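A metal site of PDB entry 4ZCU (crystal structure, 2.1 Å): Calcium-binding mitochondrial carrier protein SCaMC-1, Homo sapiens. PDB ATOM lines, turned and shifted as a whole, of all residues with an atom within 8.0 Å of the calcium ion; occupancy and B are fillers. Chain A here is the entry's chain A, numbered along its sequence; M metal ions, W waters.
Water W1 lies within hydrogen-bond range of the side-chain carboxylate (OD2) of Asp 63 (2.6 Å), the side-chain carboxylate (OD2) of Asp 67 (3.0 Å) and the side-chain amide nitrogen (ND2) of Asn 61 (3.3 Å).
N of Glu 70 is in hydrogen-bond range of OD1 of Asp 67, at 3.0 Å.
OE2 of Glu 70 lies close to N of Val 60, at 3.3 Å.
The backbone carbonyl oxygen (O) of Asp 59 is in hydrogen-bond range of the side-chain amino group (NZ) of Lys 62 (2.4 Å).
The side-chain carboxylate (OD2) of Asp 59 lies within hydrogen-bond range of the backbone NH (N) of Gly 64, 2.7 Å away.
Within 4 Å of the calcium ion: Asp 59, Asn 61, Asp 63, Lys 65 and Glu 70.
The nearest printed residue that does not touch the calcium ion is Leu 66 (4.3 Å).
The calcium ion is bound by O of Lys 65 (2.2 Å), OD1 of Asn 61 (2.3 Å), OE1 of Glu 70 (2.3 Å), OD1 of Asp 63 (2.3 Å), OD1 of Asp 59 (2.4 Å), OE2 of Glu 70 (2.4 Å) and water W1 (2.4 Å).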
ATOM      1  N   VAL A  29      24.504 -22.736 -14.950  1.00  0.00           N
ATOM      2  CA  VAL A  29      25.811 -22.142 -15.191  1.00  0.00           C
ATOM      3  C   VAL A  29      26.771 -23.159 -15.777  1.00  0.00           C
ATOM      4  O   VAL A  29      26.587 -24.370 -15.622  1.00  0.00           O
ATOM      5  CB  VAL A  29      26.430 -21.555 -13.901  1.00  0.00           C
ATOM      6  CG1 VAL A  29      25.538 -20.447 -13.344  1.00  0.00           C
ATOM      7  CG2 VAL A  29      26.673 -22.638 -12.874  1.00  0.00           C
ATOM      8  N   VAL A  30      27.800 -22.676 -16.472  1.00  0.00           N
ATOM      9  CA  VAL A  30      28.863 -23.537 -16.950  1.00  0.00           C
ATOM     10  C   VAL A  30      30.155 -23.230 -16.199  1.00  0.00           C
ATOM     11  O   VAL A  30      30.651 -22.103 -16.247  1.00  0.00           O
ATOM     12  CB  VAL A  30      29.096 -23.374 -18.465  1.00  0.00           C
ATOM     13  CG1 VAL A  30      30.329 -24.163 -18.895  1.00  0.00           C
ATOM     14  CG2 VAL A  30      27.876 -23.823 -19.245  1.00  0.00           C
ATOM     15  N   PHE A  55      36.788 -18.018 -20.852  1.00  0.00           N
ATOM     16  CA  PHE A  55      36.089 -17.957 -19.568  1.00  0.00           C
ATOM     17  C   PHE A  55      36.279 -16.600 -18.878  1.00  0.00           C
ATOM     18  O   PHE A  55      35.313 -16.026 -18.372  1.00  0.00           O
ATOM     19  CB  PHE A  55      36.567 -19.077 -18.638  1.00  0.00           C
ATOM     20  CG  PHE A  55      35.527 -19.505 -17.640  1.00  0.00           C
ATOM     21  CD1 PHE A  55      35.209 -18.710 -16.549  1.00  0.00           C
ATOM     22  CD2 PHE A  55      34.862 -20.713 -17.804  1.00  0.00           C
ATOM     23  CE1 PHE A  55      34.239 -19.101 -15.651  1.00  0.00           C
ATOM     24  CE2 PHE A  55      33.900 -21.112 -16.897  1.00  0.00           C
ATOM     25  CZ  PHE A  55      33.588 -20.306 -15.813  1.00  0.00           C
ATOM     26  N   GLY A  58      34.342 -13.954 -20.686  1.00  0.00           N
ATOM     27  CA  GLY A  58      32.916 -14.123 -20.495  1.00  0.00           C
ATOM     28  C   GLY A  58      32.397 -13.853 -19.094  1.00  0.00           C
ATOM     29  O   GLY A  58      31.269 -13.395 -18.926  1.00  0.00           O
ATOM     30  N   ASP A  59      33.212 -14.141 -18.088  1.00  0.00           N
ATOM     31  CA  ASP A  59      32.788 -13.988 -16.699  1.00  0.00           C
ATOM     32  C   ASP A  59      32.847 -12.524 -16.272  1.00  0.00           C
ATOM     33  O   ASP A  59      33.729 -12.112 -15.506  1.00  0.00           O
ATOM     34  CB  ASP A  59      33.661 -14.839 -15.776  1.00  0.00           C
ATOM     35  CG  ASP A  59      33.151 -14.881 -14.350  1.00  0.00           C
ATOM     36  OD1 ASP A  59      31.964 -14.541 -14.129  1.00  0.00           O
ATOM     37  OD2 ASP A  59      33.933 -15.240 -13.445  1.00  0.00           O
ATOM     38  N   VAL A  60      31.896 -11.735 -16.769  1.00  0.00           N
ATOM     39  CA  VAL A  60      31.877 -10.295 -16.544  1.00  0.00           C
ATOM     40  C   VAL A  60      31.735  -9.917 -15.068  1.00  0.00           C
ATOM     41  O   VAL A  60      32.398  -9.009 -14.581  1.00  0.00           O
ATOM     42  CB  VAL A  60      30.732  -9.636 -17.340  1.00  0.00           C
ATOM     43  CG1 VAL A  60      30.652  -8.142 -17.053  1.00  0.00           C
ATOM     44  CG2 VAL A  60      30.897  -9.889 -18.830  1.00  0.00           C
ATOM     45  N   ASN A  61      30.874 -10.634 -14.345  1.00  0.00           N
ATOM     46  CA  ASN A  61      30.654 -10.344 -12.934  1.00  0.00           C
ATOM     47  C   ASN A  61      31.659 -11.062 -12.033  1.00  0.00           C
ATOM     48  O   ASN A  61      31.606 -10.926 -10.810  1.00  0.00           O
ATOM     49  CB  ASN A  61      29.220 -10.706 -12.525  1.00  0.00           C
ATOM     50  CG  ASN A  61      28.966 -12.200 -12.505  1.00  0.00           C
ATOM     51  OD1 ASN A  61      29.680 -12.967 -13.153  1.00  0.00           O
ATOM     52  ND2 ASN A  61      27.943 -12.619 -11.777  1.00  0.00           N
ATOM     53  N   LYS A  62      32.582 -11.802 -12.654  1.00  0.00           N
ATOM     54  CA  LYS A  62      33.669 -12.486 -11.950  1.00  0.00           C
ATOM     55  C   LYS A  62      33.240 -13.328 -10.747  1.00  0.00           C
ATOM     56  O   LYS A  62      33.697 -13.101  -9.624  1.00  0.00           O
ATOM     57  CB  LYS A  62      34.720 -11.462 -11.488  1.00  0.00           C
ATOM     58  CG  LYS A  62      35.182 -10.486 -12.563  1.00  0.00           C
ATOM     59  CD  LYS A  62      36.334 -11.075 -13.373  1.00  0.00           C
ATOM     60  CE  LYS A  62      36.571 -10.310 -14.671  1.00  0.00           C
ATOM     61  NZ  LYS A  62      35.435 -10.419 -15.614  1.00  0.00           N
ATOM     62  N   ASP A  63      32.368 -14.299 -10.973  1.00  0.00           N
ATOM     63  CA  ASP A  63      31.978 -15.224  -9.912  1.00  0.00           C
ATOM     64  C   ASP A  63      32.517 -16.619 -10.185  1.00  0.00           C
ATOM     65  O   ASP A  63      32.203 -17.569  -9.469  1.00  0.00           O
ATOM     66  CB  ASP A  63      30.452 -15.259  -9.745  1.00  0.00           C
ATOM     67  CG  ASP A  63      29.733 -15.659 -11.018  1.00  0.00           C
ATOM     68  OD1 ASP A  63      30.392 -15.786 -12.070  1.00  0.00           O
ATOM     69  OD2 ASP A  63      28.501 -15.854 -10.958  1.00  0.00           O
ATOM     70  N   GLY A  64      33.335 -16.749 -11.231  1.00  0.00           N
ATOM     71  CA  GLY A  64      33.947 -18.024 -11.569  1.00  0.00           C
ATOM     72  C   GLY A  64      32.947 -18.929 -12.257  1.00  0.00           C
ATOM     73  O   GLY A  64      33.133 -20.141 -12.332  1.00  0.00           O
ATOM     74  N   LYS A  65      31.880 -18.324 -12.784  1.00  0.00           N
ATOM     75  CA  LYS A  65      30.822 -19.075 -13.455  1.00  0.00           C
ATOM     76  C   LYS A  65      30.312 -18.342 -14.685  1.00  0.00           C
ATOM     77  O   LYS A  65      30.244 -17.115 -14.702  1.00  0.00           O
ATOM     78  CB  LYS A  65      29.658 -19.312 -12.487  1.00  0.00           C
ATOM     79  CG  LYS A  65      29.917 -20.329 -11.395  1.00  0.00           C
ATOM     80  CD  LYS A  65      28.783 -20.315 -10.380  1.00  0.00           C
ATOM     81  CE  LYS A  65      28.644 -18.944  -9.733  1.00  0.00           C
ATOM     82  NZ  LYS A  65      27.603 -18.913  -8.678  1.00  0.00           N
ATOM     83  N   LEU A  66      29.967 -19.104 -15.720  1.00  0.00           N
ATOM     84  CA  LEU A  66      29.346 -18.518 -16.903  1.00  0.00           C
ATOM     85  C   LEU A  66      27.853 -18.831 -16.902  1.00  0.00           C
ATOM     86  O   LEU A  66      27.456 -19.974 -17.104  1.00  0.00           O
ATOM     87  CB  LEU A  66      29.975 -19.048 -18.189  1.00  0.00           C
ATOM     88  CG  LEU A  66      31.443 -18.705 -18.494  1.00  0.00           C
ATOM     89  CD1 LEU A  66      31.898 -19.415 -19.754  1.00  0.00           C
ATOM     90  CD2 LEU A  66      31.624 -17.199 -18.637  1.00  0.00           C
ATOM     91  N   ASP A  67      27.025 -17.821 -16.668  1.00  0.00           N
ATOM     92  CA  ASP A  67      25.584 -17.990 -16.822  1.00  0.00           C
ATOM     93  C   ASP A  67      25.224 -17.782 -18.287  1.00  0.00           C
ATOM     94  O   ASP A  67      26.085 -17.487 -19.112  1.00  0.00           O
ATOM     95  CB  ASP A  67      24.806 -17.058 -15.888  1.00  0.00           C
ATOM     96  CG  ASP A  67      25.152 -15.588 -16.087  1.00  0.00           C
ATOM     97  OD1 ASP A  67      25.474 -15.176 -17.221  1.00  0.00           O
ATOM     98  OD2 ASP A  67      25.085 -14.837 -15.091  1.00  0.00           O
ATOM     99  N   PHE A  68      23.950 -17.953 -18.619  1.00  0.00           N
ATOM    100  CA  PHE A  68      23.518 -17.926 -20.010  1.00  0.00           C
ATOM    101  C   PHE A  68      23.777 -16.588 -20.715  1.00  0.00           C
ATOM    102  O   PHE A  68      24.221 -16.564 -21.871  1.00  0.00           O
ATOM    103  CB  PHE A  68      22.037 -18.272 -20.113  1.00  0.00           C
ATOM    104  CG  PHE A  68      21.472 -18.114 -21.490  1.00  0.00           C
ATOM    105  CD1 PHE A  68      21.946 -18.880 -22.539  1.00  0.00           C
ATOM    106  CD2 PHE A  68      20.466 -17.190 -21.741  1.00  0.00           C
ATOM    107  CE1 PHE A  68      21.429 -18.739 -23.809  1.00  0.00           C
ATOM    108  CE2 PHE A  68      19.947 -17.038 -23.011  1.00  0.00           C
ATOM    109  CZ  PHE A  68      20.429 -17.814 -24.052  1.00  0.00           C
ATOM    110  N   GLU A  69      23.512 -15.480 -20.027  1.00  0.00           N
ATOM    111  CA  GLU A  69      23.677 -14.165 -20.645  1.00  0.00           C
ATOM    112  C   GLU A  69      25.149 -13.860 -20.933  1.00  0.00           C
ATOM    113  O   GLU A  69      25.469 -13.261 -21.959  1.00  0.00           O
ATOM    114  CB  GLU A  69      23.070 -13.054 -19.772  1.00  0.00           C
ATOM    115  CG  GLU A  69      23.697 -12.866 -18.391  1.00  0.00           C
ATOM    116  CD  GLU A  69      23.095 -11.690 -17.649  1.00  0.00           C
ATOM    117  OE1 GLU A  69      22.945 -10.610 -18.250  1.00  0.00           O
ATOM    118  OE2 GLU A  69      22.764 -11.846 -16.453  1.00  0.00           O
ATOM    119  N   GLU A  70      26.031 -14.285 -20.043  1.00  0.00           N
ATOM    120  CA  GLU A  70      27.480 -14.091 -20.217  1.00  0.00           C
ATOM    121  C   GLU A  70      27.992 -14.870 -21.433  1.00  0.00           C
ATOM    122  O   GLU A  70      28.739 -14.340 -22.251  1.00  0.00           O
ATOM    123  CB  GLU A  70      28.230 -14.518 -18.959  1.00  0.00           C
ATOM    124  CG  GLU A  70      28.110 -13.553 -17.783  1.00  0.00           C
ATOM    125  CD  GLU A  70      28.754 -14.089 -16.514  1.00  0.00           C
ATOM    126  OE1 GLU A  70      28.774 -15.325 -16.331  1.00  0.00           O
ATOM    127  OE2 GLU A  70      29.242 -13.284 -15.697  1.00  0.00           O
ATOM    128  N   PHE A  71      27.571 -16.123 -21.521  1.00  0.00           N
ATOM    129  CA  PHE A  71      27.936 -17.012 -22.617  1.00  0.00           C
ATOM    130  C   PHE A  71      27.460 -16.441 -23.958  1.00  0.00           C
ATOM    131  O   PHE A  71      28.254 -16.255 -24.902  1.00  0.00           O
ATOM    132  CB  PHE A  71      27.331 -18.401 -22.375  1.00  0.00           C
ATOM    133  CG  PHE A  71      27.761 -19.447 -23.365  1.00  0.00           C
ATOM    134  CD1 PHE A  71      29.015 -20.023 -23.278  1.00  0.00           C
ATOM    135  CD2 PHE A  71      26.895 -19.867 -24.357  1.00  0.00           C
ATOM    136  CE1 PHE A  71      29.420 -20.987 -24.188  1.00  0.00           C
ATOM    137  CE2 PHE A  71      27.287 -20.844 -25.268  1.00  0.00           C
ATOM    138  CZ  PHE A  71      28.546 -21.399 -25.187  1.00  0.00           C
HETATM  139 CA    CA M   1      29.654 -15.065 -14.177  1.00  0.00          CA
HETATM  140  O   HOH W   1      27.458 -15.513 -13.336  1.00  0.00           O
